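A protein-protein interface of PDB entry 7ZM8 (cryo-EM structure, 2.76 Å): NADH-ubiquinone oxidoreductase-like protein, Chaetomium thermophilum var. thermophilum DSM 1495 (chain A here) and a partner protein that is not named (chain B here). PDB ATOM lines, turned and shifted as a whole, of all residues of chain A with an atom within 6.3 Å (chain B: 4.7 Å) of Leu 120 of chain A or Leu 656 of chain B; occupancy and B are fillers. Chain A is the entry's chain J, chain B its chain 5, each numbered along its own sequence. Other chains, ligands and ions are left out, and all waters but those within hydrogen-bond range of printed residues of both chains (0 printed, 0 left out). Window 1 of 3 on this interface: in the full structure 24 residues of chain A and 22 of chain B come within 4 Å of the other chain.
Among the printed residues, merely in contact across the chains: Tyr 69 of chain A with Tyr 654 of chain B, Tyr 69 of chain A with Leu 657 of chain B, Thr 116 of chain A with Leu 657 of chain B, Thr 116 of chain A with Ile 660 of chain B, Val 119 of chain A with Ile 660 of chain B, Leu 120 of chain A with Leu 656 of chain B, Leu 120 of chain A with Leu 657 of chain B, Ala 123 of chain A with Tyr 652 of chain B, Ala 123 of chain A with Leu 656 of chain B, Leu 130 of chain A with Tyr 652 of chain B and Leu 130 of chain A with Leu 655 of chain B.
Of chain B, only Leu 656 and Leu 657 come within 4 Å of Leu 120 of chain A.
Printed residues of chain A within 4 Å of Leu 656 of chain B: Leu 120 (3.7 Å) and Ala 123 (3.7 Å).
Of the printed residues of chain A, Leu 655 of chain B touches Leu 130.
Of the printed residues of chain B, Ala 123 of chain A touches Tyr 652 (3.6 Å) and Leu 656 (3.7 Å).
Printed residues of chain A within 4 Å of Tyr 654 of chain B: Tyr 69.
Ala 95 of chain A touches none of the printed residues of chain B.
The nearest residue of chain B that does not touch Leu 120 of chain A is Ile 660 of chain B (4.2 Å).
The nearest residue of chain A that does not touch Leu 656 of chain B is Leu 130 of chain A (4.1 Å).
The nearest printed residue of chain A that does not touch Leu 655 of chain B is Leu 120 of chain A (6.7 Å).
The backbone NH (N) of Glu 124 of chain A lies close to the side-chain hydroxyl (OH) of Tyr 652 of chain B, at 3.5 Å.
The side-chain hydroxyl (OH) of Tyr 69 of chain A is in hydrogen-bond range of the side-chain hydroxyl (OG) of Ser 653 of chain B.
OE1 of Glu 124 of chain A sits close to OD1 of Asn 88 of chain A, 3.2 Å away.
Hydrophobic or aromatic side chains of chain B within 4 Å of the printed part of chain A: Tyr 652, Tyr 654, Leu 655, Leu 656, Leu 657 and Ile 660.
Of the 19 printed residues of chain A, 7 touch a printed residue of chain B.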
ATOM      1  N   TYR A  69      -3.805  -6.953  -1.303  1.00  0.00           N
ATOM      2  CA  TYR A  69      -4.830  -6.206  -2.020  1.00  0.00           C
ATOM      3  C   TYR A  69      -6.206  -6.445  -1.423  1.00  0.00           C
ATOM      4  O   TYR A  69      -6.924  -5.497  -1.085  1.00  0.00           O
ATOM      5  CB  TYR A  69      -4.825  -6.587  -3.499  1.00  0.00           C
ATOM      6  CG  TYR A  69      -6.114  -6.256  -4.211  1.00  0.00           C
ATOM      7  CD1 TYR A  69      -6.395  -4.959  -4.606  1.00  0.00           C
ATOM      8  CD2 TYR A  69      -7.048  -7.241  -4.488  1.00  0.00           C
ATOM      9  CE1 TYR A  69      -7.571  -4.652  -5.253  1.00  0.00           C
ATOM     10  CE2 TYR A  69      -8.225  -6.945  -5.133  1.00  0.00           C
ATOM     11  CZ  TYR A  69      -8.483  -5.650  -5.515  1.00  0.00           C
ATOM     12  OH  TYR A  69      -9.659  -5.352  -6.162  1.00  0.00           O
ATOM     13  N   TRP A  85     -15.974   2.613  -5.668  1.00  0.00           N
ATOM     14  CA  TRP A  85     -14.720   2.499  -6.402  1.00  0.00           C
ATOM     15  C   TRP A  85     -13.525   2.947  -5.583  1.00  0.00           C
ATOM     16  O   TRP A  85     -12.389   2.625  -5.946  1.00  0.00           O
ATOM     17  CB  TRP A  85     -14.784   3.330  -7.678  1.00  0.00           C
ATOM     18  CG  TRP A  85     -14.930   4.788  -7.398  1.00  0.00           C
ATOM     19  CD1 TRP A  85     -16.092   5.472  -7.210  1.00  0.00           C
ATOM     20  CD2 TRP A  85     -13.874   5.742  -7.250  1.00  0.00           C
ATOM     21  NE1 TRP A  85     -15.828   6.795  -6.963  1.00  0.00           N
ATOM     22  CE2 TRP A  85     -14.471   6.985  -6.980  1.00  0.00           C
ATOM     23  CE3 TRP A  85     -12.483   5.664  -7.319  1.00  0.00           C
ATOM     24  CZ2 TRP A  85     -13.727   8.141  -6.782  1.00  0.00           C
ATOM     25  CZ3 TRP A  85     -11.746   6.811  -7.121  1.00  0.00           C
ATOM     26  CH2 TRP A  85     -12.369   8.035  -6.858  1.00  0.00           C
ATOM     27  N   ASN A  88     -11.315   0.138  -4.117  1.00  0.00           N
ATOM     28  CA  ASN A  88     -10.420  -0.434  -5.115  1.00  0.00           C
ATOM     29  C   ASN A  88      -9.169   0.411  -5.312  1.00  0.00           C
ATOM     30  O   ASN A  88      -8.197  -0.068  -5.900  1.00  0.00           O
ATOM     31  CB  ASN A  88     -11.147  -0.605  -6.446  1.00  0.00           C
ATOM     32  CG  ASN A  88     -12.035  -1.834  -6.470  1.00  0.00           C
ATOM     33  OD1 ASN A  88     -12.624  -2.173  -7.495  1.00  0.00           O
ATOM     34  ND2 ASN A  88     -12.161  -2.491  -5.326  1.00  0.00           N
ATOM     35  N   GLY A  89      -9.178   1.655  -4.841  1.00  0.00           N
ATOM     36  CA  GLY A  89      -7.994   2.487  -4.841  1.00  0.00           C
ATOM     37  C   GLY A  89      -7.067   2.209  -3.674  1.00  0.00           C
ATOM     38  O   GLY A  89      -5.852   2.106  -3.861  1.00  0.00           O
ATOM     39  N   GLY A  91      -6.897  -0.565  -1.859  1.00  0.00           N
ATOM     40  CA  GLY A  91      -6.319  -1.884  -2.041  1.00  0.00           C
ATOM     41  C   GLY A  91      -5.242  -1.908  -3.108  1.00  0.00           C
ATOM     42  O   GLY A  91      -4.224  -2.588  -2.961  1.00  0.00           O
ATOM     43  N   GLY A  92      -5.455  -1.177  -4.202  1.00  0.00           N
ATOM     44  CA  GLY A  92      -4.458  -1.138  -5.260  1.00  0.00           C
ATOM     45  C   GLY A  92      -3.176  -0.456  -4.832  1.00  0.00           C
ATOM     46  O   GLY A  92      -2.084  -0.859  -5.240  1.00  0.00           O
ATOM     47  N   ALA A  95      -1.410  -2.920  -2.648  1.00  0.00           N
ATOM     48  CA  ALA A  95      -0.944  -4.030  -3.471  1.00  0.00           C
ATOM     49  C   ALA A  95       0.289  -3.633  -4.269  1.00  0.00           C
ATOM     50  O   ALA A  95       1.289  -4.357  -4.288  1.00  0.00           O
ATOM     51  CB  ALA A  95      -2.057  -4.496  -4.403  1.00  0.00           C
ATOM     52  N   LEU A 115       0.781   3.238 -10.085  1.00  0.00           N
ATOM     53  CA  LEU A 115       0.190   2.634 -11.272  1.00  0.00           C
ATOM     54  C   LEU A 115      -0.924   1.666 -10.904  1.00  0.00           C
ATOM     55  O   LEU A 115      -1.996   1.680 -11.519  1.00  0.00           O
ATOM     56  CB  LEU A 115       1.269   1.922 -12.086  1.00  0.00           C
ATOM     57  CG  LEU A 115       0.829   1.282 -13.404  1.00  0.00           C
ATOM     58  CD1 LEU A 115       0.314   2.334 -14.374  1.00  0.00           C
ATOM     59  CD2 LEU A 115       1.967   0.488 -14.024  1.00  0.00           C
ATOM     60  N   THR A 116      -0.689   0.820  -9.900  1.00  0.00           N
ATOM     61  CA  THR A 116      -1.683  -0.177  -9.518  1.00  0.00           C
ATOM     62  C   THR A 116      -2.934   0.471  -8.948  1.00  0.00           C
ATOM     63  O   THR A 116      -4.054   0.064  -9.273  1.00  0.00           O
ATOM     64  CB  THR A 116      -1.082  -1.153  -8.508  1.00  0.00           C
ATOM     65  OG1 THR A 116       0.231  -1.537  -8.934  1.00  0.00           O
ATOM     66  CG2 THR A 116      -1.958  -2.394  -8.377  1.00  0.00           C
ATOM     67  N   GLY A 117      -2.766   1.480  -8.096  1.00  0.00           N
ATOM     68  CA  GLY A 117      -3.921   2.121  -7.496  1.00  0.00           C
ATOM     69  C   GLY A 117      -4.782   2.846  -8.507  1.00  0.00           C
ATOM     70  O   GLY A 117      -6.013   2.790  -8.440  1.00  0.00           O
ATOM     71  N   VAL A 118      -4.150   3.542  -9.454  1.00  0.00           N
ATOM     72  CA  VAL A 118      -4.907   4.300 -10.444  1.00  0.00           C
ATOM     73  C   VAL A 118      -5.719   3.369 -11.333  1.00  0.00           C
ATOM     74  O   VAL A 118      -6.901   3.617 -11.592  1.00  0.00           O
ATOM     75  CB  VAL A 118      -3.964   5.193 -11.270  1.00  0.00           C
ATOM     76  CG1 VAL A 118      -4.737   5.899 -12.372  1.00  0.00           C
ATOM     77  CG2 VAL A 118      -3.296   6.217 -10.374  1.00  0.00           C
ATOM     78  N   VAL A 119      -5.108   2.287 -11.813  1.00  0.00           N
ATOM     79  CA  VAL A 119      -5.798   1.423 -12.765  1.00  0.00           C
ATOM     80  C   VAL A 119      -6.911   0.632 -12.086  1.00  0.00           C
ATOM     81  O   VAL A 119      -8.004   0.478 -12.643  1.00  0.00           O
ATOM     82  CB  VAL A 119      -4.790   0.511 -13.488  1.00  0.00           C
ATOM     83  CG1 VAL A 119      -4.138  -0.439 -12.523  1.00  0.00           C
ATOM     84  CG2 VAL A 119      -5.481  -0.255 -14.601  1.00  0.00           C
ATOM     85  N   LEU A 120      -6.670   0.132 -10.872  1.00  0.00           N
ATOM     86  CA  LEU A 120      -7.690  -0.666 -10.201  1.00  0.00           C
ATOM     87  C   LEU A 120      -8.869   0.186  -9.759  1.00  0.00           C
ATOM     88  O   LEU A 120      -9.978  -0.333  -9.597  1.00  0.00           O
ATOM     89  CB  LEU A 120      -7.084  -1.402  -9.010  1.00  0.00           C
ATOM     90  CG  LEU A 120      -6.094  -2.519  -9.337  1.00  0.00           C
ATOM     91  CD1 LEU A 120      -5.968  -3.450  -8.154  1.00  0.00           C
ATOM     92  CD2 LEU A 120      -6.526  -3.294 -10.568  1.00  0.00           C
ATOM     93  N   ALA A 121      -8.654   1.484  -9.553  1.00  0.00           N
ATOM     94  CA  ALA A 121      -9.770   2.372  -9.258  1.00  0.00           C
ATOM     95  C   ALA A 121     -10.448   2.851 -10.532  1.00  0.00           C
ATOM     96  O   ALA A 121     -11.667   3.042 -10.554  1.00  0.00           O
ATOM     97  CB  ALA A 121      -9.290   3.562  -8.431  1.00  0.00           C
ATOM     98  N   THR A 122      -9.667   3.063 -11.593  1.00  0.00           N
ATOM     99  CA  THR A 122     -10.225   3.514 -12.863  1.00  0.00           C
ATOM    100  C   THR A 122     -11.127   2.452 -13.472  1.00  0.00           C
ATOM    101  O   THR A 122     -12.163   2.774 -14.063  1.00  0.00           O
ATOM    102  CB  THR A 122      -9.098   3.874 -13.828  1.00  0.00           C
ATOM    103  OG1 THR A 122      -8.305   4.923 -13.260  1.00  0.00           O
ATOM    104  CG2 THR A 122      -9.654   4.335 -15.161  1.00  0.00           C
ATOM    105  N   ALA A 123     -10.747   1.181 -13.339  1.00  0.00           N
ATOM    106  CA  ALA A 123     -11.604   0.104 -13.815  1.00  0.00           C
ATOM    107  C   ALA A 123     -12.925   0.080 -13.061  1.00  0.00           C
ATOM    108  O   ALA A 123     -13.987  -0.092 -13.665  1.00  0.00           O
ATOM    109  CB  ALA A 123     -10.885  -1.234 -13.676  1.00  0.00           C
ATOM    110  N   GLU A 124     -12.882   0.263 -11.743  1.00  0.00           N
ATOM    111  CA  GLU A 124     -14.105   0.144 -10.962  1.00  0.00           C
ATOM    112  C   GLU A 124     -15.012   1.351 -11.158  1.00  0.00           C
ATOM    113  O   GLU A 124     -16.233   1.202 -11.280  1.00  0.00           O
ATOM    114  CB  GLU A 124     -13.776  -0.048  -9.486  1.00  0.00           C
ATOM    115  CG  GLU A 124     -15.007  -0.229  -8.629  1.00  0.00           C
ATOM    116  CD  GLU A 124     -15.765  -1.507  -8.954  1.00  0.00           C
ATOM    117  OE1 GLU A 124     -15.136  -2.467  -9.452  1.00  0.00           O
ATOM    118  OE2 GLU A 124     -16.993  -1.547  -8.727  1.00  0.00           O
ATOM    119  N   TYR A 125     -14.428   2.550 -11.255  1.00  0.00           N
ATOM    120  CA  TYR A 125     -15.283   3.761 -11.350  1.00  0.00           C
ATOM    121  C   TYR A 125     -15.927   3.814 -12.734  1.00  0.00           C
ATOM    122  O   TYR A 125     -17.071   4.292 -12.848  1.00  0.00           O
ATOM    123  CB  TYR A 125     -14.466   5.028 -11.101  1.00  0.00           C
ATOM    124  CG  TYR A 125     -15.278   6.296 -11.178  1.00  0.00           C
ATOM    125  CD1 TYR A 125     -16.266   6.567 -10.246  1.00  0.00           C
ATOM    126  CD2 TYR A 125     -15.070   7.221 -12.188  1.00  0.00           C
ATOM    127  CE1 TYR A 125     -17.023   7.724 -10.310  1.00  0.00           C
ATOM    128  CE2 TYR A 125     -15.819   8.384 -12.267  1.00  0.00           C
ATOM    129  CZ  TYR A 125     -16.799   8.637 -11.324  1.00  0.00           C
ATOM    130  OH  TYR A 125     -17.542   9.779 -11.390  1.00  0.00           O
ATOM    131  N   LEU A 130     -14.542  -6.002 -17.876  1.00  0.00           N
ATOM    132  CA  LEU A 130     -14.125  -7.414 -18.115  1.00  0.00           C
ATOM    133  C   LEU A 130     -15.292  -8.398 -17.967  1.00  0.00           C
ATOM    134  O   LEU A 130     -15.179  -9.511 -18.505  1.00  0.00           O
ATOM    135  CB  LEU A 130     -12.936  -7.749 -17.212  1.00  0.00           C
ATOM    136  CG  LEU A 130     -11.685  -6.907 -17.464  1.00  0.00           C
ATOM    137  CD1 LEU A 130     -10.559  -7.311 -16.528  1.00  0.00           C
ATOM    138  CD2 LEU A 130     -11.239  -7.024 -18.913  1.00  0.00           C
ATOM    139  N   TYR B 652     -13.171  -9.491 -11.613  1.00  0.00           N
ATOM    140  CA  TYR B 652     -12.368  -9.027 -12.738  1.00  0.00           C
ATOM    141  C   TYR B 652     -11.116  -8.301 -12.274  1.00  0.00           C
ATOM    142  O   TYR B 652     -10.102  -8.309 -12.980  1.00  0.00           O
ATOM    143  CB  TYR B 652     -13.207  -8.123 -13.640  1.00  0.00           C
ATOM    144  CG  TYR B 652     -13.449  -6.752 -13.059  1.00  0.00           C
ATOM    145  CD1 TYR B 652     -14.470  -6.538 -12.146  1.00  0.00           C
ATOM    146  CD2 TYR B 652     -12.660  -5.672 -13.425  1.00  0.00           C
ATOM    147  CE1 TYR B 652     -14.696  -5.290 -11.611  1.00  0.00           C
ATOM    148  CE2 TYR B 652     -12.877  -4.417 -12.894  1.00  0.00           C
ATOM    149  CZ  TYR B 652     -13.896  -4.232 -11.988  1.00  0.00           C
ATOM    150  OH  TYR B 652     -14.120  -2.987 -11.457  1.00  0.00           O
ATOM    151  N   SER B 653     -11.163  -7.668 -11.100  1.00  0.00           N
ATOM    152  CA  SER B 653      -9.987  -6.971 -10.590  1.00  0.00           C
ATOM    153  C   SER B 653      -8.843  -7.933 -10.320  1.00  0.00           C
ATOM    154  O   SER B 653      -7.674  -7.562 -10.468  1.00  0.00           O
ATOM    155  CB  SER B 653     -10.342  -6.200  -9.320  1.00  0.00           C
ATOM    156  OG  SER B 653     -10.713  -7.084  -8.278  1.00  0.00           O
ATOM    157  N   TYR B 654      -9.157  -9.169  -9.920  1.00  0.00           N
ATOM    158  CA  TYR B 654      -8.115 -10.167  -9.698  1.00  0.00           C
ATOM    159  C   TYR B 654      -7.315 -10.409 -10.967  1.00  0.00           C
ATOM    160  O   TYR B 654      -6.122 -10.725 -10.910  1.00  0.00           O
ATOM    161  CB  TYR B 654      -8.735 -11.475  -9.209  1.00  0.00           C
ATOM    162  CG  TYR B 654      -9.109 -11.481  -7.750  1.00  0.00           C
ATOM    163  CD1 TYR B 654      -8.355 -10.788  -6.815  1.00  0.00           C
ATOM    164  CD2 TYR B 654     -10.217 -12.187  -7.305  1.00  0.00           C
ATOM    165  CE1 TYR B 654      -8.696 -10.795  -5.479  1.00  0.00           C
ATOM    166  CE2 TYR B 654     -10.565 -12.199  -5.974  1.00  0.00           C
ATOM    167  CZ  TYR B 654      -9.802 -11.502  -5.065  1.00  0.00           C
ATOM    168  OH  TYR B 654     -10.149 -11.513  -3.735  1.00  0.00           O
ATOM    169  N   LEU B 655      -7.962 -10.283 -12.125  1.00  0.00           N
ATOM    170  CA  LEU B 655      -7.254 -10.420 -13.390  1.00  0.00           C
ATOM    171  C   LEU B 655      -6.285  -9.265 -13.596  1.00  0.00           C
ATOM    172  O   LEU B 655      -5.120  -9.474 -13.944  1.00  0.00           O
ATOM    173  CB  LEU B 655      -8.257 -10.501 -14.542  1.00  0.00           C
ATOM    174  CG  LEU B 655      -7.699 -10.854 -15.921  1.00  0.00           C
ATOM    175  CD1 LEU B 655      -7.024 -12.214 -15.886  1.00  0.00           C
ATOM    176  CD2 LEU B 655      -8.805 -10.833 -16.964  1.00  0.00           C
ATOM    177  N   LEU B 656      -6.748  -8.036 -13.367  1.00  0.00           N
ATOM    178  CA  LEU B 656      -5.914  -6.872 -13.635  1.00  0.00           C
ATOM    179  C   LEU B 656      -4.669  -6.870 -12.757  1.00  0.00           C
ATOM    180  O   LEU B 656      -3.579  -6.516 -13.217  1.00  0.00           O
ATOM    181  CB  LEU B 656      -6.728  -5.596 -13.439  1.00  0.00           C
ATOM    182  CG  LEU B 656      -7.613  -5.191 -14.615  1.00  0.00           C
ATOM    183  CD1 LEU B 656      -8.396  -3.933 -14.291  1.00  0.00           C
ATOM    184  CD2 LEU B 656      -6.775  -4.988 -15.862  1.00  0.00           C
ATOM    185  N   LEU B 657      -4.807  -7.279 -11.493  1.00  0.00           N
ATOM    186  CA  LEU B 657      -3.631  -7.485 -10.652  1.00  0.00           C
ATOM    187  C   LEU B 657      -2.656  -8.468 -11.279  1.00  0.00           C
ATOM    188  O   LEU B 657      -1.438  -8.294 -11.176  1.00  0.00           O
ATOM    189  CB  LEU B 657      -4.039  -7.977  -9.269  1.00  0.00           C
ATOM    190  CG  LEU B 657      -4.442  -6.941  -8.241  1.00  0.00           C
ATOM    191  CD1 LEU B 657      -4.558  -7.630  -6.913  1.00  0.00           C
ATOM    192  CD2 LEU B 657      -3.372  -5.885  -8.181  1.00  0.00           C
ATOM    193  N   ILE B 658      -3.173  -9.528 -11.901  1.00  0.00           N
ATOM    194  CA  ILE B 658      -2.305 -10.512 -12.538  1.00  0.00           C
ATOM    195  C   ILE B 658      -1.532  -9.871 -13.683  1.00  0.00           C
ATOM    196  O   ILE B 658      -0.319 -10.059 -13.815  1.00  0.00           O
ATOM    197  CB  ILE B 658      -3.135 -11.719 -13.016  1.00  0.00           C
ATOM    198  CG1 ILE B 658      -3.515 -12.607 -11.829  1.00  0.00           C
ATOM    199  CG2 ILE B 658      -2.376 -12.521 -14.060  1.00  0.00           C
ATOM    200  CD1 ILE B 658      -2.388 -13.453 -11.313  1.00  0.00           C
ATOM    201  N   ILE B 659      -2.220  -9.088 -14.517  1.00  0.00           N
ATOM    202  CA  ILE B 659      -1.576  -8.454 -15.665  1.00  0.00           C
ATOM    203  C   ILE B 659      -0.528  -7.451 -15.203  1.00  0.00           C
ATOM    204  O   ILE B 659       0.570  -7.380 -15.765  1.00  0.00           O
ATOM    205  CB  ILE B 659      -2.627  -7.792 -16.578  1.00  0.00           C
ATOM    206  CG1 ILE B 659      -3.888  -8.650 -16.699  1.00  0.00           C
ATOM    207  CG2 ILE B 659      -2.049  -7.543 -17.955  1.00  0.00           C
ATOM    208  CD1 ILE B 659      -3.643 -10.099 -17.098  1.00  0.00           C
ATOM    209  N   ILE B 660      -0.847  -6.657 -14.184  1.00  0.00           N
ATOM    210  CA  ILE B 660       0.115  -5.680 -13.687  1.00  0.00           C
ATOM    211  C   ILE B 660       1.293  -6.377 -13.020  1.00  0.00           C
ATOM    212  O   ILE B 660       2.440  -5.939 -13.149  1.00  0.00           O
ATOM    213  CB  ILE B 660      -0.570  -4.685 -12.736  1.00  0.00           C
ATOM    214  CG1 ILE B 660      -1.699  -3.960 -13.457  1.00  0.00           C
ATOM    215  CG2 ILE B 660       0.429  -3.675 -12.204  1.00  0.00           C
ATOM    216  CD1 ILE B 660      -2.846  -3.622 -12.549  1.00  0.00           C
